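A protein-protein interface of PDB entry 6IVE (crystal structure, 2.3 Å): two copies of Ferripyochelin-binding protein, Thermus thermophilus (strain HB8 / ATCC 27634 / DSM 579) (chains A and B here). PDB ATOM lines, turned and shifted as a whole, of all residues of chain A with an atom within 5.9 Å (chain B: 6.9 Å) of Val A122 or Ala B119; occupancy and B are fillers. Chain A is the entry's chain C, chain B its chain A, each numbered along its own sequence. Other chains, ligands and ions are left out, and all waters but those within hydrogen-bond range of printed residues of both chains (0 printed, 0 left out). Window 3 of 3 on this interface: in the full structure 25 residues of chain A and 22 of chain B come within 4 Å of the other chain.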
ATOM      1  N   ALA A 103      -0.736  -6.652   9.599  1.00  0.00           N
ATOM      2  CA  ALA A 103      -1.526  -5.878   8.655  1.00  0.00           C
ATOM      3  C   ALA A 103      -2.109  -4.635   9.327  1.00  0.00           C
ATOM      4  O   ALA A 103      -2.115  -4.496  10.554  1.00  0.00           O
ATOM      5  CB  ALA A 103      -2.646  -6.734   8.062  1.00  0.00           C
ATOM      6  N   VAL A 104      -2.594  -3.711   8.496  1.00  0.00           N
ATOM      7  CA  VAL A 104      -3.262  -2.498   8.953  1.00  0.00           C
ATOM      8  C   VAL A 104      -4.558  -2.340   8.170  1.00  0.00           C
ATOM      9  O   VAL A 104      -4.556  -2.417   6.936  1.00  0.00           O
ATOM     10  CB  VAL A 104      -2.376  -1.247   8.783  1.00  0.00           C
ATOM     11  CG1 VAL A 104      -3.078  -0.016   9.352  1.00  0.00           C
ATOM     12  CG2 VAL A 104      -1.016  -1.447   9.442  1.00  0.00           C
ATOM     13  N   VAL A 105      -5.660  -2.114   8.884  1.00  0.00           N
ATOM     14  CA  VAL A 105      -6.975  -1.920   8.283  1.00  0.00           C
ATOM     15  C   VAL A 105      -7.524  -0.589   8.787  1.00  0.00           C
ATOM     16  O   VAL A 105      -7.734  -0.420   9.995  1.00  0.00           O
ATOM     17  CB  VAL A 105      -7.935  -3.074   8.618  1.00  0.00           C
ATOM     18  CG1 VAL A 105      -9.286  -2.855   7.963  1.00  0.00           C
ATOM     19  CG2 VAL A 105      -7.337  -4.408   8.180  1.00  0.00           C
ATOM     20  N   LEU A 106      -7.768   0.345   7.867  1.00  0.00           N
ATOM     21  CA  LEU A 106      -8.022   1.737   8.212  1.00  0.00           C
ATOM     22  C   LEU A 106      -9.521   2.046   8.241  1.00  0.00           C
ATOM     23  O   LEU A 106     -10.371   1.192   7.975  1.00  0.00           O
ATOM     24  CB  LEU A 106      -7.276   2.651   7.239  1.00  0.00           C
ATOM     25  CG  LEU A 106      -5.757   2.462   7.280  1.00  0.00           C
ATOM     26  CD1 LEU A 106      -5.081   3.083   6.068  1.00  0.00           C
ATOM     27  CD2 LEU A 106      -5.190   3.040   8.566  1.00  0.00           C
ATOM     28  N   VAL A 117      -7.264 -10.810   5.090  1.00  0.00           N
ATOM     29  CA  VAL A 117      -6.314  -9.742   4.806  1.00  0.00           C
ATOM     30  C   VAL A 117      -4.911 -10.319   4.926  1.00  0.00           C
ATOM     31  O   VAL A 117      -4.561 -10.909   5.956  1.00  0.00           O
ATOM     32  CB  VAL A 117      -6.507  -8.555   5.765  1.00  0.00           C
ATOM     33  CG1 VAL A 117      -5.494  -7.459   5.460  1.00  0.00           C
ATOM     34  CG2 VAL A 117      -7.925  -8.016   5.672  1.00  0.00           C
ATOM     35  N   GLY A 118      -4.110 -10.155   3.877  1.00  0.00           N
ATOM     36  CA  GLY A 118      -2.773 -10.715   3.880  1.00  0.00           C
ATOM     37  C   GLY A 118      -1.886 -10.079   4.933  1.00  0.00           C
ATOM     38  O   GLY A 118      -2.085  -8.936   5.347  1.00  0.00           O
ATOM     39  N   GLY A 120       0.857  -8.089   6.673  1.00  0.00           N
ATOM     40  CA  GLY A 120       1.527  -6.864   6.292  1.00  0.00           C
ATOM     41  C   GLY A 120       0.771  -5.992   5.315  1.00  0.00           C
ATOM     42  O   GLY A 120       1.268  -4.916   4.962  1.00  0.00           O
ATOM     43  N   ALA A 121      -0.407  -6.416   4.863  1.00  0.00           N
ATOM     44  CA  ALA A 121      -1.177  -5.611   3.929  1.00  0.00           C
ATOM     45  C   ALA A 121      -1.776  -4.400   4.634  1.00  0.00           C
ATOM     46  O   ALA A 121      -2.123  -4.448   5.818  1.00  0.00           O
ATOM     47  CB  ALA A 121      -2.289  -6.444   3.289  1.00  0.00           C
ATOM     48  N   VAL A 122      -1.894  -3.305   3.894  1.00  0.00           N
ATOM     49  CA  VAL A 122      -2.511  -2.082   4.393  1.00  0.00           C
ATOM     50  C   VAL A 122      -3.787  -1.867   3.592  1.00  0.00           C
ATOM     51  O   VAL A 122      -3.739  -1.618   2.381  1.00  0.00           O
ATOM     52  CB  VAL A 122      -1.566  -0.877   4.292  1.00  0.00           C
ATOM     53  CG1 VAL A 122      -2.277   0.398   4.727  1.00  0.00           C
ATOM     54  CG2 VAL A 122      -0.327  -1.111   5.143  1.00  0.00           C
ATOM     55  N   VAL A 123      -4.928  -1.976   4.265  1.00  0.00           N
ATOM     56  CA  VAL A 123      -6.237  -1.872   3.618  1.00  0.00           C
ATOM     57  C   VAL A 123      -6.672  -0.408   3.692  1.00  0.00           C
ATOM     58  O   VAL A 123      -6.960   0.082   4.795  1.00  0.00           O
ATOM     59  CB  VAL A 123      -7.262  -2.794   4.286  1.00  0.00           C
ATOM     60  CG1 VAL A 123      -8.647  -2.573   3.693  1.00  0.00           C
ATOM     61  CG2 VAL A 123      -6.833  -4.244   4.135  1.00  0.00           C
ATOM     62  N   PRO A 124      -6.742   0.303   2.567  1.00  0.00           N
ATOM     63  CA  PRO A 124      -7.012   1.749   2.603  1.00  0.00           C
ATOM     64  C   PRO A 124      -8.361   2.049   3.233  1.00  0.00           C
ATOM     65  O   PRO A 124      -9.208   1.153   3.366  1.00  0.00           O
ATOM     66  CB  PRO A 124      -6.993   2.146   1.118  1.00  0.00           C
ATOM     67  CG  PRO A 124      -6.210   1.074   0.445  1.00  0.00           C
ATOM     68  CD  PRO A 124      -6.515  -0.184   1.198  1.00  0.00           C
ATOM     69  N   MET A 127     -12.060   0.665   1.880  1.00  0.00           N
ATOM     70  CA  MET A 127     -11.975  -0.479   0.984  1.00  0.00           C
ATOM     71  C   MET A 127     -12.873  -1.605   1.474  1.00  0.00           C
ATOM     72  O   MET A 127     -12.938  -1.895   2.672  1.00  0.00           O
ATOM     73  CB  MET A 127     -10.535  -0.980   0.865  1.00  0.00           C
ATOM     74  CG  MET A 127     -10.429  -2.359   0.214  1.00  0.00           C
ATOM     75  SD  MET A 127      -8.785  -2.811  -0.364  1.00  0.00           S
ATOM     76  CE  MET A 127      -8.511  -1.570  -1.626  1.00  0.00           C
ATOM     77  N   GLY A 137      -0.969  -6.771  -0.158  1.00  0.00           N
ATOM     78  CA  GLY A 137      -0.131  -5.759  -0.766  1.00  0.00           C
ATOM     79  C   GLY A 137      -0.238  -4.421  -0.052  1.00  0.00           C
ATOM     80  O   GLY A 137      -1.060  -4.212   0.841  1.00  0.00           O
ATOM     81  N   VAL A 138       0.636  -3.508  -0.468  1.00  0.00           N
ATOM     82  CA  VAL A 138       0.615  -2.136   0.025  1.00  0.00           C
ATOM     83  C   VAL A 138       0.496  -1.175  -1.157  1.00  0.00           C
ATOM     84  O   VAL A 138       1.479  -0.933  -1.856  1.00  0.00           O
ATOM     85  CB  VAL A 138       1.869  -1.812   0.867  1.00  0.00           C
ATOM     86  CG1 VAL A 138       1.726  -0.447   1.527  1.00  0.00           C
ATOM     87  CG2 VAL A 138       2.115  -2.893   1.909  1.00  0.00           C
ATOM     88  N   PRO A 139      -0.709  -0.630  -1.393  1.00  0.00           N
ATOM     89  CA  PRO A 139      -1.938  -0.890  -0.636  1.00  0.00           C
ATOM     90  C   PRO A 139      -2.586  -2.214  -1.019  1.00  0.00           C
ATOM     91  O   PRO A 139      -2.244  -2.783  -2.054  1.00  0.00           O
ATOM     92  CB  PRO A 139      -2.837   0.285  -1.023  1.00  0.00           C
ATOM     93  CG  PRO A 139      -2.419   0.608  -2.414  1.00  0.00           C
ATOM     94  CD  PRO A 139      -0.931   0.349  -2.472  1.00  0.00           C
ATOM     95  N   ALA A 140      -3.508  -2.691  -0.189  1.00  0.00           N
ATOM     96  CA  ALA A 140      -4.116  -3.994  -0.413  1.00  0.00           C
ATOM     97  C   ALA A 140      -4.969  -3.991  -1.675  1.00  0.00           C
ATOM     98  O   ALA A 140      -5.575  -2.982  -2.045  1.00  0.00           O
ATOM     99  CB  ALA A 140      -4.968  -4.398   0.790  1.00  0.00           C
ATOM    100  N   ARG B  85       1.270   1.771  16.725  1.00  0.00           N
ATOM    101  CA  ARG B  85       2.197   0.747  16.248  1.00  0.00           C
ATOM    102  C   ARG B  85       3.211   1.294  15.242  1.00  0.00           C
ATOM    103  O   ARG B  85       3.773   0.536  14.447  1.00  0.00           O
ATOM    104  CB  ARG B  85       1.431  -0.434  15.639  1.00  0.00           C
ATOM    105  CG  ARG B  85       2.162  -1.766  15.656  1.00  0.00           C
ATOM    106  CD  ARG B  85       1.691  -2.638  14.500  1.00  0.00           C
ATOM    107  NE  ARG B  85       2.242  -2.191  13.223  1.00  0.00           N
ATOM    108  CZ  ARG B  85       1.784  -2.569  12.032  1.00  0.00           C
ATOM    109  NH1 ARG B  85       0.753  -3.398  11.949  1.00  0.00           N
ATOM    110  NH2 ARG B  85       2.351  -2.113  10.923  1.00  0.00           N
ATOM    111  N   VAL B  99       2.961  10.750  11.564  1.00  0.00           N
ATOM    112  CA  VAL B  99       3.529   9.477  11.134  1.00  0.00           C
ATOM    113  C   VAL B  99       2.421   8.440  11.244  1.00  0.00           C
ATOM    114  O   VAL B  99       2.009   8.072  12.351  1.00  0.00           O
ATOM    115  CB  VAL B  99       4.755   9.085  11.968  1.00  0.00           C
ATOM    116  CG1 VAL B  99       5.230   7.693  11.574  1.00  0.00           C
ATOM    117  CG2 VAL B  99       5.865  10.103  11.782  1.00  0.00           C
ATOM    118  N   GLY B 100       1.936   7.973  10.095  1.00  0.00           N
ATOM    119  CA  GLY B 100       0.751   7.136  10.072  1.00  0.00           C
ATOM    120  C   GLY B 100       0.921   5.857  10.866  1.00  0.00           C
ATOM    121  O   GLY B 100       2.028   5.365  11.093  1.00  0.00           O
ATOM    122  N   MET B 101      -0.213   5.316  11.295  1.00  0.00           N
ATOM    123  CA  MET B 101      -0.198   4.116  12.115  1.00  0.00           C
ATOM    124  C   MET B 101       0.406   2.955  11.333  1.00  0.00           C
ATOM    125  O   MET B 101       0.115   2.756  10.151  1.00  0.00           O
ATOM    126  CB  MET B 101      -1.615   3.782  12.593  1.00  0.00           C
ATOM    127  CG  MET B 101      -2.626   3.508  11.488  1.00  0.00           C
ATOM    128  SD  MET B 101      -4.297   3.250  12.131  1.00  0.00           S
ATOM    129  CE  MET B 101      -4.966   4.911  12.012  1.00  0.00           C
ATOM    130  N   GLY B 102       1.288   2.208  11.995  1.00  0.00           N
ATOM    131  CA  GLY B 102       1.984   1.111  11.361  1.00  0.00           C
ATOM    132  C   GLY B 102       3.155   1.503  10.487  1.00  0.00           C
ATOM    133  O   GLY B 102       3.789   0.618   9.899  1.00  0.00           O
ATOM    134  N   ALA B 103       3.467   2.790  10.378  1.00  0.00           N
ATOM    135  CA  ALA B 103       4.568   3.223   9.535  1.00  0.00           C
ATOM    136  C   ALA B 103       5.903   3.040  10.249  1.00  0.00           C
ATOM    137  O   ALA B 103       5.970   2.864  11.469  1.00  0.00           O
ATOM    138  CB  ALA B 103       4.392   4.686   9.126  1.00  0.00           C
ATOM    139  N   VAL B 116       2.606  14.194   6.016  1.00  0.00           N
ATOM    140  CA  VAL B 116       1.953  12.953   6.407  1.00  0.00           C
ATOM    141  C   VAL B 116       2.757  11.777   5.874  1.00  0.00           C
ATOM    142  O   VAL B 116       3.038  11.704   4.673  1.00  0.00           O
ATOM    143  CB  VAL B 116       0.502  12.875   5.896  1.00  0.00           C
ATOM    144  CG1 VAL B 116      -0.100  11.516   6.230  1.00  0.00           C
ATOM    145  CG2 VAL B 116      -0.331  13.984   6.504  1.00  0.00           C
ATOM    146  N   VAL B 117       3.128  10.867   6.768  1.00  0.00           N
ATOM    147  CA  VAL B 117       3.636   9.554   6.386  1.00  0.00           C
ATOM    148  C   VAL B 117       2.457   8.591   6.400  1.00  0.00           C
ATOM    149  O   VAL B 117       1.826   8.388   7.443  1.00  0.00           O
ATOM    150  CB  VAL B 117       4.748   9.085   7.337  1.00  0.00           C
ATOM    151  CG1 VAL B 117       5.192   7.673   6.980  1.00  0.00           C
ATOM    152  CG2 VAL B 117       5.924  10.045   7.290  1.00  0.00           C
ATOM    153  N   GLY B 118       2.145   8.016   5.243  1.00  0.00           N
ATOM    154  CA  GLY B 118       0.989   7.149   5.143  1.00  0.00           C
ATOM    155  C   GLY B 118       1.091   5.942   6.054  1.00  0.00           C
ATOM    156  O   GLY B 118       2.174   5.519   6.464  1.00  0.00           O
ATOM    157  N   ALA B 119      -0.076   5.391   6.383  1.00  0.00           N
ATOM    158  CA  ALA B 119      -0.145   4.199   7.217  1.00  0.00           C
ATOM    159  C   ALA B 119       0.664   3.065   6.599  1.00  0.00           C
ATOM    160  O   ALA B 119       0.572   2.798   5.398  1.00  0.00           O
ATOM    161  CB  ALA B 119      -1.601   3.769   7.402  1.00  0.00           C
ATOM    162  N   GLY B 120       1.471   2.407   7.428  1.00  0.00           N
ATOM    163  CA  GLY B 120       2.272   1.287   6.984  1.00  0.00           C
ATOM    164  C   GLY B 120       3.389   1.623   6.024  1.00  0.00           C
ATOM    165  O   GLY B 120       4.038   0.700   5.516  1.00  0.00           O
ATOM    166  N   ALA B 121       3.638   2.899   5.747  1.00  0.00           N
ATOM    167  CA  ALA B 121       4.725   3.273   4.857  1.00  0.00           C
ATOM    168  C   ALA B 121       6.063   3.169   5.579  1.00  0.00           C
ATOM    169  O   ALA B 121       6.152   3.344   6.796  1.00  0.00           O
ATOM    170  CB  ALA B 121       4.527   4.693   4.328  1.00  0.00           C
ATOM    171  N   VAL B 122       7.110   2.877   4.814  1.00  0.00           N
ATOM    172  CA  VAL B 122       8.463   2.741   5.342  1.00  0.00           C
ATOM    173  C   VAL B 122       9.308   3.842   4.717  1.00  0.00           C
ATOM    174  O   VAL B 122       9.579   3.816   3.509  1.00  0.00           O
ATOM    175  CB  VAL B 122       9.057   1.352   5.059  1.00  0.00           C
ATOM    176  CG1 VAL B 122      10.543   1.324   5.385  1.00  0.00           C
ATOM    177  CG2 VAL B 122       8.318   0.293   5.861  1.00  0.00           C
ATOM    178  N   LEU B 134       2.363  14.293   1.349  1.00  0.00           N
ATOM    179  CA  LEU B 134       2.062  12.916   1.710  1.00  0.00           C
ATOM    180  C   LEU B 134       3.078  11.979   1.071  1.00  0.00           C
ATOM    181  O   LEU B 134       3.303  12.030  -0.142  1.00  0.00           O
ATOM    182  CB  LEU B 134       0.648  12.534   1.267  1.00  0.00           C
ATOM    183  CG  LEU B 134       0.317  11.041   1.273  1.00  0.00           C
ATOM    184  CD1 LEU B 134       0.329  10.482   2.688  1.00  0.00           C
ATOM    185  CD2 LEU B 134      -1.025  10.792   0.609  1.00  0.00           C
ATOM    186  N   ALA B 135       3.684  11.126   1.890  1.00  0.00           N
ATOM    187  CA  ALA B 135       4.599  10.092   1.429  1.00  0.00           C
ATOM    188  C   ALA B 135       4.017   8.737   1.794  1.00  0.00           C
ATOM    189  O   ALA B 135       3.634   8.517   2.948  1.00  0.00           O
ATOM    190  CB  ALA B 135       5.989  10.263   2.049  1.00  0.00           C
ATOM    191  N   LEU B 136       3.942   7.833   0.819  1.00  0.00           N
ATOM    192  CA  LEU B 136       3.386   6.516   1.089  1.00  0.00           C
ATOM    193  C   LEU B 136       4.103   5.466   0.255  1.00  0.00           C
ATOM    194  O   LEU B 136       4.721   5.767  -0.769  1.00  0.00           O
ATOM    195  CB  LEU B 136       1.869   6.481   0.835  1.00  0.00           C
ATOM    196  CG  LEU B 136       1.268   6.911  -0.507  1.00  0.00           C
ATOM    197  CD1 LEU B 136       1.439   5.852  -1.590  1.00  0.00           C
ATOM    198  CD2 LEU B 136      -0.202   7.246  -0.324  1.00  0.00           C
ATOM    199  N   GLY B 137       4.011   4.225   0.714  1.00  0.00           N
ATOM    200  CA  GLY B 137       4.549   3.084   0.003  1.00  0.00           C
ATOM    201  C   GLY B 137       5.672   2.407   0.766  1.00  0.00           C
ATOM    202  O   GLY B 137       6.155   2.884   1.792  1.00  0.00           O
ATOM    203  N   VAL B 138       6.072   1.256   0.230  1.00  0.00           N
ATOM    204  CA  VAL B 138       7.218   0.512   0.735  1.00  0.00           C
ATOM    205  C   VAL B 138       8.158   0.211  -0.429  1.00  0.00           C
ATOM    206  O   VAL B 138       7.917  -0.722  -1.196  1.00  0.00           O
ATOM    207  CB  VAL B 138       6.792  -0.785   1.445  1.00  0.00           C
ATOM    208  CG1 VAL B 138       8.019  -1.550   1.928  1.00  0.00           C
ATOM    209  CG2 VAL B 138       5.852  -0.480   2.606  1.00  0.00           C
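The backbone carbonyl oxygen of Ala A103 sits at hydrogen-bond distance from the guanidinium group of Arg B85, 3.4 Å away.
The backbone carbonyl oxygen of Met B101 lies within hydrogen-bond range of the backbone NH of Gly B120, 3.1 Å away.
O of Val A104 lies within hydrogen-bond range of N of Val A123 (2.7 Å).
The backbone carbonyl oxygen of Ala A121 is in hydrogen-bond range of the backbone NH of Val A104 (2.8 Å).
The backbone NH (N) of Val A122 sits at hydrogen-bond distance from the backbone carbonyl oxygen (O) of Gly A137 (3.3 Å).
O of Gly B102 lies within hydrogen-bond range of NH2 of Arg B85 (3.3 Å).
O of Val A122 sits at hydrogen-bond distance from N of Ala A140, 2.8 Å away.
Among the printed residues, merely in contact across the chains: Val A104 with Arg B85, Leu A106 with Met B101, Val A122 with Ala B119, Leu A106 with Ala B119 and Val A122 with Gly B120.
Of the printed residues of chain B, Val A122 touches Ala B119 and Gly B120.
Ala B119 touches two residues of chain A.
Printed residues of chain B within 4 Å of Val A104: Arg B85 (3.6 Å).
Printed residues of chain B within 4 Å of Ala A103: Arg B85.
Ala B121 touches none of the printed residues of chain A.
The nearest printed residue of chain B that does not touch Val A122 is Ala B121 (5.7 Å).
The nearest printed residue of chain B that does not touch Ala A103 is Gly B102 (7.0 Å).
Of the 16 printed residues of chain A, 4 touch a printed residue of chain B.
Printed residues of chain A that touch a printed residue of chain B: Ala A103, Val A104, Leu A106 and Val A122.
Hydrophobic or aromatic side chains of chain B within 4 Å of the printed part of chain A: Met B101 and Ala B119.
Among the printed residues, no Asp or Glu carboxylate lies within 4 Å of a Lys or Arg side-chain nitrogen of the other chain.
Val A122 touches Gly B120, but with the chains exchanged Gly A120 does not touch Val B122 (8.8 Å).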
